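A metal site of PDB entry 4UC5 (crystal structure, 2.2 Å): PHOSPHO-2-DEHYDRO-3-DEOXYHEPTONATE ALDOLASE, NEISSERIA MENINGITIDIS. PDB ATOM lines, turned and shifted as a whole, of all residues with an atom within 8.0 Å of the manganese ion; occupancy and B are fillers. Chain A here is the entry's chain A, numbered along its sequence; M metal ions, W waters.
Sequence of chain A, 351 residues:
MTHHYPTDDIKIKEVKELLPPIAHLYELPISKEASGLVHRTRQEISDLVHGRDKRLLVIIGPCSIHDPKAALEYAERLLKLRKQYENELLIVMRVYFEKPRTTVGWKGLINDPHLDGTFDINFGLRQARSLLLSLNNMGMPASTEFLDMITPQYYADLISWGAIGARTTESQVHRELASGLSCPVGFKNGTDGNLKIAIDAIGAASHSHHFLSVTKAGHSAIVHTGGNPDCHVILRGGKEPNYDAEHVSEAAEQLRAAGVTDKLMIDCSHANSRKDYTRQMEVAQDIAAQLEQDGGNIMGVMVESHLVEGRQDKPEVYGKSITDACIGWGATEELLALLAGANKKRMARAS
Merely in contact with the manganese ion: Arg 94. Five residues have an atom within 4 Å of the manganese ion: Cys 63, Arg 94, His 270, Glu 304 and Asp 324. Along chain A the residues within 4 Å of the manganese ion span positions 63 to 324. The nearest printed residue that does not touch the manganese ion is Lys 99 (4.1 Å).
The side-chain carboxylate of Asp 324 is in salt-bridge range of the side-chain amino group of Lys 99, at 3.3 Å. The side-chain sulfur (SG) of Cys 63 lies close to the side-chain hydroxyl (OG1) of Thr 323, at 3.0 Å. NE of Arg 94 is in hydrogen-bond range of O of Pro 62, 2.8 Å away. The backbone carbonyl oxygen of Asp 324 sits at hydrogen-bond distance from the side-chain hydroxyl of Ser 321 (2.6 Å). The backbone NH (N) of Cys 63 sits at hydrogen-bond distance from the side-chain sulfur (SG) of Cys 326 (3.6 Å). NH1 of Arg 94 is in hydrogen-bond range of SD of Met 302, 3.7 Å away. O of Cys 63 is in hydrogen-bond range of NH2 of Arg 94, 2.7 Å away. OE1 of Glu 304 sits at hydrogen-bond distance from OG of Ser 269, at 2.8 Å.
Water W1 binds the manganese ion. The side-chain carboxylate (OD2) of Asp 324 is bound to the manganese ion (2.0 Å). The manganese ion is bound by OE2 of Glu 304 (2.2 Å). NE2 of His 270 is bound to the manganese ion. The manganese ion is bound by the side-chain sulfur (SG) of Cys 63 (2.6 Å). The manganese ion has five donor atoms within binding distance.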
ATOM      1  N   GLY A  61      -7.344  16.461  27.217  1.00  0.00           N
ATOM      2  CA  GLY A  61      -7.748  15.066  27.194  1.00  0.00           C
ATOM      3  C   GLY A  61      -7.203  14.374  25.969  1.00  0.00           C
ATOM      4  O   GLY A  61      -6.488  15.000  25.160  1.00  0.00           O
ATOM      5  N   PRO A  62      -7.496  13.083  25.812  1.00  0.00           N
ATOM      6  CA  PRO A  62      -7.110  12.299  24.662  1.00  0.00           C
ATOM      7  C   PRO A  62      -7.509  12.942  23.324  1.00  0.00           C
ATOM      8  O   PRO A  62      -8.453  13.731  23.261  1.00  0.00           O
ATOM      9  CB  PRO A  62      -7.892  10.991  24.854  1.00  0.00           C
ATOM     10  CG  PRO A  62      -7.970  10.854  26.340  1.00  0.00           C
ATOM     11  CD  PRO A  62      -8.174  12.251  26.832  1.00  0.00           C
ATOM     12  N   CYS A  63      -6.770  12.632  22.279  1.00  0.00           N
ATOM     13  CA  CYS A  63      -7.120  13.109  20.951  1.00  0.00           C
ATOM     14  C   CYS A  63      -8.478  12.492  20.632  1.00  0.00           C
ATOM     15  O   CYS A  63      -9.360  13.191  20.141  1.00  0.00           O
ATOM     16  CB  CYS A  63      -6.075  12.723  19.920  1.00  0.00           C
ATOM     17  SG  CYS A  63      -6.575  12.952  18.200  1.00  0.00           S
ATOM     18  N   SER A  64      -8.606  11.192  20.937  1.00  0.00           N
ATOM     19  CA  SER A  64      -9.881  10.479  20.809  1.00  0.00           C
ATOM     20  C   SER A  64     -10.058   9.440  21.935  1.00  0.00           C
ATOM     21  O   SER A  64      -9.072   8.916  22.491  1.00  0.00           O
ATOM     22  CB  SER A  64      -9.965   9.778  19.449  1.00  0.00           C
ATOM     23  OG  SER A  64      -9.071   8.678  19.385  1.00  0.00           O
ATOM     24  N   ARG A  94     -11.372  16.668  27.379  1.00  0.00           N
ATOM     25  CA  ARG A  94     -11.625  16.404  25.989  1.00  0.00           C
ATOM     26  C   ARG A  94     -12.251  15.028  25.886  1.00  0.00           C
ATOM     27  O   ARG A  94     -11.630  14.027  26.231  1.00  0.00           O
ATOM     28  CB  ARG A  94     -10.292  16.379  25.247  1.00  0.00           C
ATOM     29  CG  ARG A  94     -10.232  17.262  24.024  1.00  0.00           C
ATOM     30  CD  ARG A  94      -8.875  17.128  23.345  1.00  0.00           C
ATOM     31  NE  ARG A  94      -8.937  16.276  22.171  1.00  0.00           N
ATOM     32  CZ  ARG A  94      -8.951  16.737  20.927  1.00  0.00           C
ATOM     33  NH1 ARG A  94      -8.914  18.033  20.705  1.00  0.00           N
ATOM     34  NH2 ARG A  94      -9.009  15.895  19.902  1.00  0.00           N
ATOM     35  N   TYR A  96     -13.605  13.452  22.705  1.00  0.00           N
ATOM     36  CA  TYR A  96     -13.846  13.352  21.280  1.00  0.00           C
ATOM     37  C   TYR A  96     -13.948  11.890  20.938  1.00  0.00           C
ATOM     38  O   TYR A  96     -13.070  11.124  21.307  1.00  0.00           O
ATOM     39  CB  TYR A  96     -12.694  13.978  20.497  1.00  0.00           C
ATOM     40  CG  TYR A  96     -12.635  15.480  20.503  1.00  0.00           C
ATOM     41  CD1 TYR A  96     -12.900  16.202  21.642  1.00  0.00           C
ATOM     42  CD2 TYR A  96     -12.316  16.196  19.336  1.00  0.00           C
ATOM     43  CE1 TYR A  96     -12.824  17.589  21.649  1.00  0.00           C
ATOM     44  CE2 TYR A  96     -12.225  17.575  19.332  1.00  0.00           C
ATOM     45  CZ  TYR A  96     -12.481  18.259  20.495  1.00  0.00           C
ATOM     46  OH  TYR A  96     -12.418  19.637  20.527  1.00  0.00           O
ATOM     47  N   GLU A  98     -14.198  10.726  17.714  1.00  0.00           N
ATOM     48  CA  GLU A  98     -13.651  10.475  16.392  1.00  0.00           C
ATOM     49  C   GLU A  98     -12.684  11.603  15.976  1.00  0.00           C
ATOM     50  O   GLU A  98     -12.992  12.788  16.151  1.00  0.00           O
ATOM     51  CB  GLU A  98     -14.796  10.383  15.378  1.00  0.00           C
ATOM     52  CG  GLU A  98     -14.365  10.253  13.916  1.00  0.00           C
ATOM     53  CD  GLU A  98     -15.545  10.044  12.961  1.00  0.00           C
ATOM     54  OE1 GLU A  98     -16.724  10.134  13.396  1.00  0.00           O
ATOM     55  OE2 GLU A  98     -15.298   9.767  11.771  1.00  0.00           O
ATOM     56  N   LYS A  99     -11.537  11.208  15.434  1.00  0.00           N
ATOM     57  CA  LYS A  99     -10.723  12.112  14.641  1.00  0.00           C
ATOM     58  C   LYS A  99     -11.141  11.963  13.176  1.00  0.00           C
ATOM     59  O   LYS A  99     -11.090  10.860  12.619  1.00  0.00           O
ATOM     60  CB  LYS A  99      -9.234  11.799  14.792  1.00  0.00           C
ATOM     61  CG  LYS A  99      -8.318  12.912  14.280  1.00  0.00           C
ATOM     62  CD  LYS A  99      -6.963  12.363  13.846  1.00  0.00           C
ATOM     63  CE  LYS A  99      -6.195  13.337  12.953  1.00  0.00           C
ATOM     64  NZ  LYS A  99      -6.039  14.692  13.566  1.00  0.00           N
ATOM     65  N   PRO A 100     -11.575  13.052  12.536  1.00  0.00           N
ATOM     66  CA  PRO A 100     -11.837  12.934  11.097  1.00  0.00           C
ATOM     67  C   PRO A 100     -10.532  12.755  10.342  1.00  0.00           C
ATOM     68  O   PRO A 100      -9.495  13.328  10.719  1.00  0.00           O
ATOM     69  CB  PRO A 100     -12.494  14.268  10.744  1.00  0.00           C
ATOM     70  CG  PRO A 100     -12.047  15.222  11.792  1.00  0.00           C
ATOM     71  CD  PRO A 100     -11.814  14.422  13.039  1.00  0.00           C
ATOM     72  N   GLU A 145     -16.425  17.274  19.855  1.00  0.00           N
ATOM     73  CA  GLU A 145     -16.591  17.854  18.532  1.00  0.00           C
ATOM     74  C   GLU A 145     -17.786  17.225  17.885  1.00  0.00           C
ATOM     75  O   GLU A 145     -17.904  16.029  17.842  1.00  0.00           O
ATOM     76  CB  GLU A 145     -15.386  17.588  17.612  1.00  0.00           C
ATOM     77  CG  GLU A 145     -15.561  18.273  16.254  1.00  0.00           C
ATOM     78  CD  GLU A 145     -14.415  18.052  15.273  1.00  0.00           C
ATOM     79  OE1 GLU A 145     -13.409  17.381  15.595  1.00  0.00           O
ATOM     80  OE2 GLU A 145     -14.542  18.582  14.138  1.00  0.00           O
ATOM     81  N   LYS A 188     -12.381  26.456  14.959  1.00  0.00           N
ATOM     82  CA  LYS A 188     -10.981  26.462  14.607  1.00  0.00           C
ATOM     83  C   LYS A 188     -10.715  27.197  13.314  1.00  0.00           C
ATOM     84  O   LYS A 188     -11.551  27.160  12.386  1.00  0.00           O
ATOM     85  CB  LYS A 188     -10.460  25.029  14.488  1.00  0.00           C
ATOM     86  CG  LYS A 188     -10.194  24.427  15.854  1.00  0.00           C
ATOM     87  CD  LYS A 188      -9.738  22.978  15.789  1.00  0.00           C
ATOM     88  CE  LYS A 188      -8.877  22.684  17.010  1.00  0.00           C
ATOM     89  NZ  LYS A 188      -8.472  21.257  17.159  1.00  0.00           N
ATOM     90  N   ASP A 267      -4.682  26.262  20.631  1.00  0.00           N
ATOM     91  CA  ASP A 267      -4.430  24.810  20.624  1.00  0.00           C
ATOM     92  C   ASP A 267      -2.928  24.614  20.628  1.00  0.00           C
ATOM     93  O   ASP A 267      -2.229  25.128  19.752  1.00  0.00           O
ATOM     94  CB  ASP A 267      -5.055  24.190  19.371  1.00  0.00           C
ATOM     95  CG  ASP A 267      -5.042  22.649  19.364  1.00  0.00           C
ATOM     96  OD1 ASP A 267      -4.393  22.027  20.186  1.00  0.00           O
ATOM     97  OD2 ASP A 267      -5.670  22.042  18.472  1.00  0.00           O
ATOM     98  N   SER A 269      -1.582  21.674  20.345  1.00  0.00           N
ATOM     99  CA  SER A 269      -1.295  20.478  19.567  1.00  0.00           C
ATOM    100  C   SER A 269      -1.529  20.765  18.097  1.00  0.00           C
ATOM    101  O   SER A 269      -1.596  21.934  17.678  1.00  0.00           O
ATOM    102  CB  SER A 269      -2.171  19.320  20.038  1.00  0.00           C
ATOM    103  OG  SER A 269      -1.803  18.098  19.430  1.00  0.00           O
ATOM    104  N   HIS A 270      -1.633  19.693  17.317  1.00  0.00           N
ATOM    105  CA  HIS A 270      -1.931  19.764  15.887  1.00  0.00           C
ATOM    106  C   HIS A 270      -0.912  20.571  15.079  1.00  0.00           C
ATOM    107  O   HIS A 270       0.254  20.277  15.142  1.00  0.00           O
ATOM    108  CB  HIS A 270      -3.384  20.197  15.654  1.00  0.00           C
ATOM    109  CG  HIS A 270      -4.370  19.257  16.292  1.00  0.00           C
ATOM    110  ND1 HIS A 270      -5.171  19.634  17.350  1.00  0.00           N
ATOM    111  CD2 HIS A 270      -4.668  17.971  16.030  1.00  0.00           C
ATOM    112  CE1 HIS A 270      -5.913  18.607  17.717  1.00  0.00           C
ATOM    113  NE2 HIS A 270      -5.624  17.586  16.937  1.00  0.00           N
ATOM    114  N   MET A 302      -5.975  24.497  24.458  1.00  0.00           N
ATOM    115  CA  MET A 302      -6.321  23.120  24.142  1.00  0.00           C
ATOM    116  C   MET A 302      -5.055  22.280  24.167  1.00  0.00           C
ATOM    117  O   MET A 302      -4.025  22.710  23.667  1.00  0.00           O
ATOM    118  CB  MET A 302      -6.960  23.049  22.762  1.00  0.00           C
ATOM    119  CG  MET A 302      -7.646  21.724  22.481  1.00  0.00           C
ATOM    120  SD  MET A 302      -8.739  21.759  21.006  1.00  0.00           S
ATOM    121  CE  MET A 302      -9.641  23.265  21.346  1.00  0.00           C
ATOM    122  N   GLU A 304      -3.568  18.005  24.047  1.00  0.00           N
ATOM    123  CA  GLU A 304      -3.865  16.598  23.804  1.00  0.00           C
ATOM    124  C   GLU A 304      -3.005  15.761  24.712  1.00  0.00           C
ATOM    125  O   GLU A 304      -1.790  15.685  24.524  1.00  0.00           O
ATOM    126  CB  GLU A 304      -3.660  16.239  22.355  1.00  0.00           C
ATOM    127  CG  GLU A 304      -4.742  16.830  21.463  1.00  0.00           C
ATOM    128  CD  GLU A 304      -4.787  16.224  20.065  1.00  0.00           C
ATOM    129  OE1 GLU A 304      -3.741  16.117  19.383  1.00  0.00           O
ATOM    130  OE2 GLU A 304      -5.902  15.880  19.665  1.00  0.00           O
ATOM    131  N   SER A 321      -2.962   6.716  23.032  1.00  0.00           N
ATOM    132  CA  SER A 321      -3.759   7.153  21.865  1.00  0.00           C
ATOM    133  C   SER A 321      -3.606   6.259  20.628  1.00  0.00           C
ATOM    134  O   SER A 321      -2.519   5.729  20.351  1.00  0.00           O
ATOM    135  CB  SER A 321      -3.365   8.597  21.518  1.00  0.00           C
ATOM    136  OG  SER A 321      -4.256   9.183  20.593  1.00  0.00           O
ATOM    137  N   THR A 323      -5.068   7.662  17.766  1.00  0.00           N
ATOM    138  CA  THR A 323      -5.112   8.707  16.760  1.00  0.00           C
ATOM    139  C   THR A 323      -3.855   9.558  16.946  1.00  0.00           C
ATOM    140  O   THR A 323      -2.760   8.999  16.965  1.00  0.00           O
ATOM    141  CB  THR A 323      -6.468   9.450  16.779  1.00  0.00           C
ATOM    142  OG1 THR A 323      -6.776   9.970  18.091  1.00  0.00           O
ATOM    143  CG2 THR A 323      -7.543   8.476  16.342  1.00  0.00           C
ATOM    144  N   ASP A 324      -3.981  10.876  17.119  1.00  0.00           N
ATOM    145  CA  ASP A 324      -2.798  11.729  17.312  1.00  0.00           C
ATOM    146  C   ASP A 324      -2.017  11.346  18.565  1.00  0.00           C
ATOM    147  O   ASP A 324      -2.601  10.841  19.520  1.00  0.00           O
ATOM    148  CB  ASP A 324      -3.167  13.211  17.397  1.00  0.00           C
ATOM    149  CG  ASP A 324      -3.841  13.692  16.142  1.00  0.00           C
ATOM    150  OD1 ASP A 324      -3.616  13.066  15.097  1.00  0.00           O
ATOM    151  OD2 ASP A 324      -4.616  14.678  16.216  1.00  0.00           O
ATOM    152  N   ALA A 325      -0.708  11.615  18.542  1.00  0.00           N
ATOM    153  CA  ALA A 325       0.142  11.393  19.709  1.00  0.00           C
ATOM    154  C   ALA A 325      -0.101  12.452  20.806  1.00  0.00           C
ATOM    155  O   ALA A 325      -0.235  13.650  20.516  1.00  0.00           O
ATOM    156  CB  ALA A 325       1.617  11.382  19.305  1.00  0.00           C
ATOM    157  N   CYS A 326      -0.189  11.978  22.049  1.00  0.00           N
ATOM    158  CA  CYS A 326      -0.440  12.850  23.205  1.00  0.00           C
ATOM    159  C   CYS A 326       0.735  12.828  24.180  1.00  0.00           C
ATOM    160  O   CYS A 326       1.569  11.936  24.171  1.00  0.00           O
ATOM    161  CB  CYS A 326      -1.710  12.411  23.944  1.00  0.00           C
ATOM    162  SG  CYS A 326      -3.237  12.363  22.965  1.00  0.00           S
HETATM  163 MN    MN M   1      -5.988  15.353  17.564  1.00  0.00          MN
HETATM  164  O   HOH W   1      -7.764  15.485  16.702  1.00  0.00           O
